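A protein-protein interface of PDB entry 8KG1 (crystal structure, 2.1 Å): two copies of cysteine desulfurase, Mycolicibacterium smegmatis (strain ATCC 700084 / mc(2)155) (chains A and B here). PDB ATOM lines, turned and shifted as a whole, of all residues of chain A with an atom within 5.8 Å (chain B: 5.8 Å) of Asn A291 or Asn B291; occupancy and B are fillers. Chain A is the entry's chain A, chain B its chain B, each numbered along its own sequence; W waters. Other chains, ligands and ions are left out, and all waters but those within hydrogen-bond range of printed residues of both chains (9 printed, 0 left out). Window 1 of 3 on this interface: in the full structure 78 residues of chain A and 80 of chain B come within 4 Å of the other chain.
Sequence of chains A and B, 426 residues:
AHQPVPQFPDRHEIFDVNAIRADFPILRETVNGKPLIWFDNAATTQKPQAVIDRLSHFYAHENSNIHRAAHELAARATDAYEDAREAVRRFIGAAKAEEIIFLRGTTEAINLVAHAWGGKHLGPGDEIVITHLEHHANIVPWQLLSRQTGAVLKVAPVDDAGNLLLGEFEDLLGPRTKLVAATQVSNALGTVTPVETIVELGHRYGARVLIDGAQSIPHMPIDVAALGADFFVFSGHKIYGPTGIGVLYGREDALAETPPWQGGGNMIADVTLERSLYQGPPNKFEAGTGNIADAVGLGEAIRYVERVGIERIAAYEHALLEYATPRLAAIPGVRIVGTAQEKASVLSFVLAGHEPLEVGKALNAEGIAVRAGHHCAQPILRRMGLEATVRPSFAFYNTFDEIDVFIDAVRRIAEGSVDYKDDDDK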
ATOM      1  N   TYR A  59      10.971   8.986  23.197  1.00  0.00           N
ATOM      2  CA  TYR A  59       9.920   9.856  23.716  1.00  0.00           C
ATOM      3  C   TYR A  59       9.062   9.155  24.761  1.00  0.00           C
ATOM      4  O   TYR A  59       8.533   9.811  25.666  1.00  0.00           O
ATOM      5  CB  TYR A  59       9.043  10.382  22.573  1.00  0.00           C
ATOM      6  CG  TYR A  59       9.712  11.509  21.815  1.00  0.00           C
ATOM      7  CD1 TYR A  59      10.143  12.647  22.482  1.00  0.00           C
ATOM      8  CD2 TYR A  59       9.935  11.425  20.447  1.00  0.00           C
ATOM      9  CE1 TYR A  59      10.781  13.684  21.806  1.00  0.00           C
ATOM     10  CE2 TYR A  59      10.570  12.460  19.754  1.00  0.00           C
ATOM     11  CZ  TYR A  59      10.977  13.583  20.439  1.00  0.00           C
ATOM     12  OH  TYR A  59      11.599  14.613  19.780  1.00  0.00           O
ATOM     13  N   TYR A  81      22.241  10.476  24.588  1.00  0.00           N
ATOM     14  CA  TYR A  81      22.879  11.548  23.827  1.00  0.00           C
ATOM     15  C   TYR A  81      24.384  11.311  23.703  1.00  0.00           C
ATOM     16  O   TYR A  81      24.955  11.442  22.611  1.00  0.00           O
ATOM     17  CB  TYR A  81      22.592  12.891  24.504  1.00  0.00           C
ATOM     18  CG  TYR A  81      22.739  14.132  23.643  1.00  0.00           C
ATOM     19  CD1 TYR A  81      22.248  14.183  22.340  1.00  0.00           C
ATOM     20  CD2 TYR A  81      23.351  15.267  24.156  1.00  0.00           C
ATOM     21  CE1 TYR A  81      22.378  15.343  21.571  1.00  0.00           C
ATOM     22  CE2 TYR A  81      23.487  16.420  23.409  1.00  0.00           C
ATOM     23  CZ  TYR A  81      22.994  16.462  22.123  1.00  0.00           C
ATOM     24  OH  TYR A  81      23.142  17.622  21.394  1.00  0.00           O
ATOM     25  N   ARG A 104      21.921  21.348  13.085  1.00  0.00           N
ATOM     26  CA  ARG A 104      20.763  20.892  12.308  1.00  0.00           C
ATOM     27  C   ARG A 104      21.158  20.119  11.042  1.00  0.00           C
ATOM     28  O   ARG A 104      20.437  19.197  10.631  1.00  0.00           O
ATOM     29  CB  ARG A 104      19.856  22.077  11.944  1.00  0.00           C
ATOM     30  CG  ARG A 104      18.802  21.739  10.838  1.00  0.00           C
ATOM     31  CD  ARG A 104      17.610  22.730  10.726  1.00  0.00           C
ATOM     32  NE  ARG A 104      18.080  24.102  10.541  1.00  0.00           N
ATOM     33  CZ  ARG A 104      18.296  24.961  11.535  1.00  0.00           C
ATOM     34  NH1 ARG A 104      17.907  24.693  12.774  1.00  0.00           N
ATOM     35  NH2 ARG A 104      18.907  26.120  11.280  1.00  0.00           N
ATOM     36  N   THR A 243      15.323  13.881  10.141  1.00  0.00           N
ATOM     37  CA  THR A 243      15.562  15.266   9.772  1.00  0.00           C
ATOM     38  C   THR A 243      15.981  16.053  11.010  1.00  0.00           C
ATOM     39  O   THR A 243      15.822  15.606  12.150  1.00  0.00           O
ATOM     40  CB  THR A 243      14.311  15.913   9.142  1.00  0.00           C
ATOM     41  OG1 THR A 243      13.232  15.946  10.093  1.00  0.00           O
ATOM     42  CG2 THR A 243      13.852  15.158   7.900  1.00  0.00           C
ATOM     43  N   GLY A 244      16.545  17.228  10.772  1.00  0.00           N
ATOM     44  CA  GLY A 244      16.811  18.154  11.846  1.00  0.00           C
ATOM     45  C   GLY A 244      18.093  17.925  12.602  1.00  0.00           C
ATOM     46  O   GLY A 244      18.322  18.618  13.603  1.00  0.00           O
ATOM     47  N   ILE A 245      18.934  16.984  12.166  1.00  0.00           N
ATOM     48  CA  ILE A 245      20.175  16.665  12.865  1.00  0.00           C
ATOM     49  C   ILE A 245      21.299  16.501  11.843  1.00  0.00           C
ATOM     50  O   ILE A 245      21.121  15.888  10.783  1.00  0.00           O
ATOM     51  CB  ILE A 245      20.020  15.405  13.753  1.00  0.00           C
ATOM     52  CG1 ILE A 245      21.283  15.151  14.594  1.00  0.00           C
ATOM     53  CG2 ILE A 245      19.655  14.169  12.920  1.00  0.00           C
ATOM     54  CD1 ILE A 245      21.466  16.149  15.738  1.00  0.00           C
ATOM     55  N   THR A 289      19.039  23.994  24.283  1.00  0.00           N
ATOM     56  CA  THR A 289      18.680  22.582  24.291  1.00  0.00           C
ATOM     57  C   THR A 289      19.017  21.953  22.947  1.00  0.00           C
ATOM     58  O   THR A 289      18.562  22.428  21.900  1.00  0.00           O
ATOM     59  CB  THR A 289      17.188  22.439  24.585  1.00  0.00           C
ATOM     60  OG1 THR A 289      16.904  23.040  25.856  1.00  0.00           O
ATOM     61  CG2 THR A 289      16.764  20.972  24.587  1.00  0.00           C
ATOM     62  N   GLY A 290      19.802  20.885  22.975  1.00  0.00           N
ATOM     63  CA  GLY A 290      20.111  20.165  21.758  1.00  0.00           C
ATOM     64  C   GLY A 290      18.907  19.406  21.228  1.00  0.00           C
ATOM     65  O   GLY A 290      17.895  19.200  21.908  1.00  0.00           O
ATOM     66  N   ASN A 291      19.024  18.976  19.972  1.00  0.00           N
ATOM     67  CA  ASN A 291      18.005  18.125  19.365  1.00  0.00           C
ATOM     68  C   ASN A 291      18.294  16.694  19.810  1.00  0.00           C
ATOM     69  O   ASN A 291      18.824  15.868  19.065  1.00  0.00           O
ATOM     70  CB  ASN A 291      18.009  18.267  17.853  1.00  0.00           C
ATOM     71  CG  ASN A 291      16.911  17.456  17.198  1.00  0.00           C
ATOM     72  OD1 ASN A 291      16.207  16.694  17.875  1.00  0.00           O
ATOM     73  ND2 ASN A 291      16.727  17.639  15.881  1.00  0.00           N
ATOM     74  N   ILE A 292      17.919  16.397  21.059  1.00  0.00           N
ATOM     75  CA  ILE A 292      18.366  15.153  21.688  1.00  0.00           C
ATOM     76  C   ILE A 292      17.771  13.941  20.974  1.00  0.00           C
ATOM     77  O   ILE A 292      18.496  12.997  20.617  1.00  0.00           O
ATOM     78  CB  ILE A 292      18.038  15.165  23.192  1.00  0.00           C
ATOM     79  CG1 ILE A 292      18.798  16.305  23.881  1.00  0.00           C
ATOM     80  CG2 ILE A 292      18.471  13.870  23.858  1.00  0.00           C
ATOM     81  CD1 ILE A 292      18.047  16.899  25.061  1.00  0.00           C
ATOM     82  N   ALA A 293      16.451  13.957  20.731  1.00  0.00           N
ATOM     83  CA  ALA A 293      15.803  12.784  20.142  1.00  0.00           C
ATOM     84  C   ALA A 293      16.387  12.454  18.778  1.00  0.00           C
ATOM     85  O   ALA A 293      16.629  11.285  18.466  1.00  0.00           O
ATOM     86  CB  ALA A 293      14.290  12.999  20.018  1.00  0.00           C
ATOM     87  N   ASP A 294      16.628  13.462  17.943  1.00  0.00           N
ATOM     88  CA  ASP A 294      17.067  13.113  16.597  1.00  0.00           C
ATOM     89  C   ASP A 294      18.531  12.725  16.556  1.00  0.00           C
ATOM     90  O   ASP A 294      18.919  11.931  15.701  1.00  0.00           O
ATOM     91  CB  ASP A 294      16.810  14.253  15.624  1.00  0.00           C
ATOM     92  CG  ASP A 294      15.335  14.523  15.445  1.00  0.00           C
ATOM     93  OD1 ASP A 294      14.511  13.567  15.570  1.00  0.00           O
ATOM     94  OD2 ASP A 294      14.999  15.713  15.278  1.00  0.00           O
ATOM     95  N   ALA A 295      19.361  13.261  17.457  1.00  0.00           N
ATOM     96  CA  ALA A 295      20.714  12.725  17.597  1.00  0.00           C
ATOM     97  C   ALA A 295      20.674  11.248  17.974  1.00  0.00           C
ATOM     98  O   ALA A 295      21.430  10.429  17.427  1.00  0.00           O
ATOM     99  CB  ALA A 295      21.499  13.523  18.646  1.00  0.00           C
ATOM    100  N   VAL A 296      19.799  10.887  18.919  1.00  0.00           N
ATOM    101  CA  VAL A 296      19.660   9.479  19.296  1.00  0.00           C
ATOM    102  C   VAL A 296      19.192   8.640  18.099  1.00  0.00           C
ATOM    103  O   VAL A 296      19.689   7.526  17.851  1.00  0.00           O
ATOM    104  CB  VAL A 296      18.702   9.366  20.499  1.00  0.00           C
ATOM    105  CG1 VAL A 296      18.331   7.910  20.768  1.00  0.00           C
ATOM    106  CG2 VAL A 296      19.355   9.993  21.733  1.00  0.00           C
ATOM    107  N   TYR B  59       7.377   9.543   9.106  1.00  0.00           N
ATOM    108  CA  TYR B  59       8.522   8.812   8.583  1.00  0.00           C
ATOM    109  C   TYR B  59       8.091   7.593   7.776  1.00  0.00           C
ATOM    110  O   TYR B  59       8.797   7.196   6.836  1.00  0.00           O
ATOM    111  CB  TYR B  59       9.460   8.428   9.732  1.00  0.00           C
ATOM    112  CG  TYR B  59      10.321   9.607  10.165  1.00  0.00           C
ATOM    113  CD1 TYR B  59      11.093  10.295   9.234  1.00  0.00           C
ATOM    114  CD2 TYR B  59      10.352  10.032  11.487  1.00  0.00           C
ATOM    115  CE1 TYR B  59      11.900  11.380   9.607  1.00  0.00           C
ATOM    116  CE2 TYR B  59      11.157  11.115  11.884  1.00  0.00           C
ATOM    117  CZ  TYR B  59      11.932  11.779  10.939  1.00  0.00           C
ATOM    118  OH  TYR B  59      12.730  12.853  11.299  1.00  0.00           O
ATOM    119  N   TYR B  81       4.165  20.083   6.002  1.00  0.00           N
ATOM    120  CA  TYR B  81       4.987  21.206   6.470  1.00  0.00           C
ATOM    121  C   TYR B  81       4.205  22.520   6.443  1.00  0.00           C
ATOM    122  O   TYR B  81       4.257  23.311   7.397  1.00  0.00           O
ATOM    123  CB  TYR B  81       6.237  21.320   5.594  1.00  0.00           C
ATOM    124  CG  TYR B  81       7.433  22.077   6.174  1.00  0.00           C
ATOM    125  CD1 TYR B  81       7.854  21.864   7.485  1.00  0.00           C
ATOM    126  CD2 TYR B  81       8.176  22.952   5.382  1.00  0.00           C
ATOM    127  CE1 TYR B  81       8.965  22.518   8.005  1.00  0.00           C
ATOM    128  CE2 TYR B  81       9.300  23.616   5.889  1.00  0.00           C
ATOM    129  CZ  TYR B  81       9.684  23.389   7.204  1.00  0.00           C
ATOM    130  OH  TYR B  81      10.783  24.021   7.735  1.00  0.00           O
ATOM    131  N   ARG B 104      15.716  25.700  15.326  1.00  0.00           N
ATOM    132  CA  ARG B 104      15.877  24.631  16.316  1.00  0.00           C
ATOM    133  C   ARG B 104      15.148  24.923  17.623  1.00  0.00           C
ATOM    134  O   ARG B 104      14.648  23.998  18.283  1.00  0.00           O
ATOM    135  CB  ARG B 104      17.363  24.386  16.613  1.00  0.00           C
ATOM    136  CG  ARG B 104      17.593  23.285  17.688  1.00  0.00           C
ATOM    137  CD  ARG B 104      19.061  22.823  17.771  1.00  0.00           C
ATOM    138  NE  ARG B 104      20.008  23.925  17.618  1.00  0.00           N
ATOM    139  CZ  ARG B 104      20.705  24.169  16.511  1.00  0.00           C
ATOM    140  NH1 ARG B 104      20.619  23.379  15.445  1.00  0.00           N
ATOM    141  NH2 ARG B 104      21.497  25.238  16.464  1.00  0.00           N
ATOM    142  N   THR B 243      11.779  17.504  20.275  1.00  0.00           N
ATOM    143  CA  THR B 243      12.987  18.305  20.355  1.00  0.00           C
ATOM    144  C   THR B 243      13.386  18.771  18.952  1.00  0.00           C
ATOM    145  O   THR B 243      12.857  18.311  17.932  1.00  0.00           O
ATOM    146  CB  THR B 243      14.147  17.526  20.992  1.00  0.00           C
ATOM    147  OG1 THR B 243      14.434  16.371  20.201  1.00  0.00           O
ATOM    148  CG2 THR B 243      13.800  17.062  22.411  1.00  0.00           C
ATOM    149  N   GLY B 244      14.326  19.702  18.911  1.00  0.00           N
ATOM    150  CA  GLY B 244      14.892  20.152  17.657  1.00  0.00           C
ATOM    151  C   GLY B 244      14.042  21.107  16.845  1.00  0.00           C
ATOM    152  O   GLY B 244      14.391  21.373  15.690  1.00  0.00           O
ATOM    153  N   ILE B 245      12.944  21.636  17.391  1.00  0.00           N
ATOM    154  CA  ILE B 245      12.084  22.548  16.635  1.00  0.00           C
ATOM    155  C   ILE B 245      11.652  23.700  17.530  1.00  0.00           C
ATOM    156  O   ILE B 245      11.332  23.515  18.709  1.00  0.00           O
ATOM    157  CB  ILE B 245      10.861  21.823  16.014  1.00  0.00           C
ATOM    158  CG1 ILE B 245      10.149  22.739  15.008  1.00  0.00           C
ATOM    159  CG2 ILE B 245       9.889  21.280  17.090  1.00  0.00           C
ATOM    160  CD1 ILE B 245      10.920  22.877  13.685  1.00  0.00           C
ATOM    161  N   THR B 289      17.870  22.036   4.307  1.00  0.00           N
ATOM    162  CA  THR B 289      16.714  21.186   4.571  1.00  0.00           C
ATOM    163  C   THR B 289      16.142  21.517   5.941  1.00  0.00           C
ATOM    164  O   THR B 289      16.855  21.505   6.949  1.00  0.00           O
ATOM    165  CB  THR B 289      17.112  19.706   4.502  1.00  0.00           C
ATOM    166  OG1 THR B 289      17.657  19.422   3.210  1.00  0.00           O
ATOM    167  CG2 THR B 289      15.908  18.768   4.763  1.00  0.00           C
ATOM    168  N   GLY B 290      14.866  21.844   5.982  1.00  0.00           N
ATOM    169  CA  GLY B 290      14.239  22.098   7.255  1.00  0.00           C
ATOM    170  C   GLY B 290      14.023  20.820   8.039  1.00  0.00           C
ATOM    171  O   GLY B 290      14.060  19.705   7.510  1.00  0.00           O
ATOM    172  N   ASN B 291      13.799  20.995   9.340  1.00  0.00           N
ATOM    173  CA  ASN B 291      13.413  19.889  10.204  1.00  0.00           C
ATOM    174  C   ASN B 291      11.925  19.606   9.996  1.00  0.00           C
ATOM    175  O   ASN B 291      11.073  19.896  10.839  1.00  0.00           O
ATOM    176  CB  ASN B 291      13.727  20.211  11.656  1.00  0.00           C
ATOM    177  CG  ASN B 291      13.552  19.018  12.545  1.00  0.00           C
ATOM    178  OD1 ASN B 291      13.094  17.951  12.094  1.00  0.00           O
ATOM    179  ND2 ASN B 291      13.916  19.171  13.825  1.00  0.00           N
ATOM    180  N   ILE B 292      11.622  19.008   8.840  1.00  0.00           N
ATOM    181  CA  ILE B 292      10.226  18.826   8.441  1.00  0.00           C
ATOM    182  C   ILE B 292       9.474  17.995   9.474  1.00  0.00           C
ATOM    183  O   ILE B 292       8.356  18.335   9.878  1.00  0.00           O
ATOM    184  CB  ILE B 292      10.137  18.174   7.046  1.00  0.00           C
ATOM    185  CG1 ILE B 292      11.015  18.910   6.032  1.00  0.00           C
ATOM    186  CG2 ILE B 292       8.704  18.191   6.551  1.00  0.00           C
ATOM    187  CD1 ILE B 292      10.517  20.280   5.720  1.00  0.00           C
ATOM    188  N   ALA B 293      10.066  16.866   9.891  1.00  0.00           N
ATOM    189  CA  ALA B 293       9.331  15.927  10.735  1.00  0.00           C
ATOM    190  C   ALA B 293       8.970  16.547  12.077  1.00  0.00           C
ATOM    191  O   ALA B 293       7.851  16.367  12.576  1.00  0.00           O
ATOM    192  CB  ALA B 293      10.152  14.653  10.948  1.00  0.00           C
ATOM    193  N   ASP B 294       9.906  17.267  12.692  1.00  0.00           N
ATOM    194  CA  ASP B 294       9.611  17.805  14.016  1.00  0.00           C
ATOM    195  C   ASP B 294       8.661  18.987  13.946  1.00  0.00           C
ATOM    196  O   ASP B 294       7.886  19.208  14.881  1.00  0.00           O
ATOM    197  CB  ASP B 294      10.891  18.211  14.727  1.00  0.00           C
ATOM    198  CG  ASP B 294      11.758  17.018  15.046  1.00  0.00           C
ATOM    199  OD1 ASP B 294      11.197  15.907  15.266  1.00  0.00           O
ATOM    200  OD2 ASP B 294      12.988  17.203  15.091  1.00  0.00           O
ATOM    201  N   ALA B 295       8.699  19.748  12.853  1.00  0.00           N
ATOM    202  CA  ALA B 295       7.671  20.760  12.642  1.00  0.00           C
ATOM    203  C   ALA B 295       6.292  20.115  12.524  1.00  0.00           C
ATOM    204  O   ALA B 295       5.317  20.603  13.109  1.00  0.00           O
ATOM    205  CB  ALA B 295       8.003  21.576  11.392  1.00  0.00           C
ATOM    206  N   VAL B 296       6.196  18.998  11.794  1.00  0.00           N
ATOM    207  CA  VAL B 296       4.923  18.265  11.718  1.00  0.00           C
ATOM    208  C   VAL B 296       4.481  17.806  13.112  1.00  0.00           C
ATOM    209  O   VAL B 296       3.306  17.952  13.501  1.00  0.00           O
ATOM    210  CB  VAL B 296       5.053  17.084  10.730  1.00  0.00           C
ATOM    211  CG1 VAL B 296       3.864  16.173  10.826  1.00  0.00           C
ATOM    212  CG2 VAL B 296       5.210  17.601   9.270  1.00  0.00           C
HETATM  213  O   HOH W   1      19.760  20.339  15.579  1.00  0.00           O
HETATM  214  O   HOH W   2      19.926  24.245  20.508  1.00  0.00           O
HETATM  215  O   HOH W   3      16.897  18.193   8.282  1.00  0.00           O
HETATM  216  O   HOH W   4      18.318  23.742   7.765  1.00  0.00           O
HETATM  217  O   HOH W   5      17.487  21.232  14.583  1.00  0.00           O
HETATM  218  O   HOH W   6      12.058  14.030  17.043  1.00  0.00           O
HETATM  219  O   HOH W   7      15.452  20.749  21.220  1.00  0.00           O
HETATM  220  O   HOH W   8      15.521  22.890  13.268  1.00  0.00           O
HETATM  221  O   HOH W   9      12.397  13.725  13.879  1.00  0.00           O
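The backbone carbonyl oxygen (O) of Gly B244 lies within hydrogen-bond range of the side-chain amide nitrogen (ND2) of Asn B291 (2.9 Å).
The side-chain carboxylate of Asp A294 lies within hydrogen-bond range of the side-chain amide nitrogen of Asn A291, at 2.7 Å.
The side-chain carboxylate of Asp B294 lies within hydrogen-bond range of the side-chain amide nitrogen of Asn B291 (2.5 Å).
The backbone NH of Ile A245 lies close to the backbone carbonyl oxygen of Arg A104 (3.1 Å).
The side-chain amide nitrogen (ND2) of Asn A291 sits at hydrogen-bond distance from the backbone carbonyl oxygen (O) of Gly A244.
The backbone carbonyl oxygen (O) of Arg B104 is in hydrogen-bond range of the backbone NH (N) of Ile B245.
Thr A243 touches Ile B292.
Gly A244 touches Asn B291.
CA of Gly B244 touches CG of Asn A291, 3.4 Å away.
Asn B291 touches Asn A291.
OD2 of Asp B294 touches ND2 of Asn A291 (3.8 Å).
Thr B243 touches Ile A292 (OG1 to N, 3.6 Å).
Asp A294 touches Asn B291.
Of the 14 printed residues of chain B, 8 touch a printed residue of chain A.
Hydrophobic or aromatic side chains of chain A within 4 Å of the printed part of chain B: Tyr A59 and Ala A293.
Among the printed residues, no Asp or Glu carboxylate lies within 4 Å of a Lys or Arg side-chain nitrogen of the other chain.
OH of Tyr A59 is in hydrogen-bond range of N of Thr B243 (2.9 Å).
N of Ala A293 lies within hydrogen-bond range of OG1 of Thr B243.
The side-chain carboxylate (OD2) of Asp B294 sits close to the side-chain carboxylate (OD2) of Asp A294, at 2.5 Å.
The side-chain amide oxygen (OD1) of Asn A291 lies within hydrogen-bond range of the side-chain hydroxyl (OG1) of Thr B243, at 2.9 Å.
The backbone NH (N) of Thr A243 lies within hydrogen-bond range of the side-chain hydroxyl (OH) of Tyr B59.
The backbone NH of Ala B293 lies within hydrogen-bond range of the side-chain hydroxyl of Thr A243, 3.3 Å away.
OG1 of Thr A243 is in hydrogen-bond range of OD1 of Asn B291 (2.8 Å).
The guanidinium group (NH1) of Arg B104 lies close to the backbone NH (N) of Arg A104, 3.4 Å away.
Thr A243 touches Asn B291, and with the chains exchanged Asn A291 touches Thr B243.
Thr A243 touches Ala B293, and with the chains exchanged Ala A293 touches Thr B243.
Gly A244 touches Asn B291, and with the chains exchanged Asn A291 touches Gly B244.
Asn A291 touches Asp B294, and with the chains exchanged Asp A294 touches Asn B291.
Positions printed for both chains: 59, 81, 104, 243, 244, 245, 289, 290, 291, 292, 293, 294, 295 and 296.
Of the 15 pairs that touch across the chains among the printed residues, 15 have their exchanged pair printed and touching as well.
Of chain B, only Thr B243, Gly B244, Asn B291 and Asp B294 come within 4 Å of Asn A291.
Asn B291 touches just these residues of chain A: Thr A243 (2.8 Å), Gly A244 (3.4 Å), Asn A291 (3.8 Å) and Asp A294 (3.9 Å).
Of the printed residues of chain A, Arg B104 touches Arg A104 (3.4 Å).
Of the printed residues of chain A, Ile B292 touches Thr A243.
Of the printed residues of chain B, Ile A292 touches Thr B243.
Printed residues of chain A within 4 Å of Gly B244: Asn A291 (3.4 Å).
The nearest residue of chain A that does not touch Asn B291 is Arg A104 (4.4 Å).
The nearest printed residue of chain A that does not touch Arg B104 is Thr A289 (4.2 Å).
Water W2 lies within hydrogen-bond range of O of Thr A289 (2.7 Å) and NE of Arg B104 (2.9 Å).
Water W3 bridges N of Gly A244 and O of Gly B290.
Water W9 lies within hydrogen-bond range of the side-chain carboxylate (OD1) of Asp A294 (2.7 Å), the side-chain hydroxyl (OH) of Tyr B59 (2.7 Å) and the side-chain carboxylate (OD1) of Asp B294 (2.9 Å).
Water W7 bridges the backbone NH of Gly B244 (2.8 Å) and the backbone carbonyl oxygen of Gly A290 (3.0 Å).
Water W5 bridges the backbone carbonyl oxygen of Gly A244 and the backbone carbonyl oxygen of Gly B244.
Water W1 lies within hydrogen-bond range of O of Gly A244 (3.0 Å), NH1 of Arg B104 (3.2 Å) and N of Arg A104 (3.5 Å).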
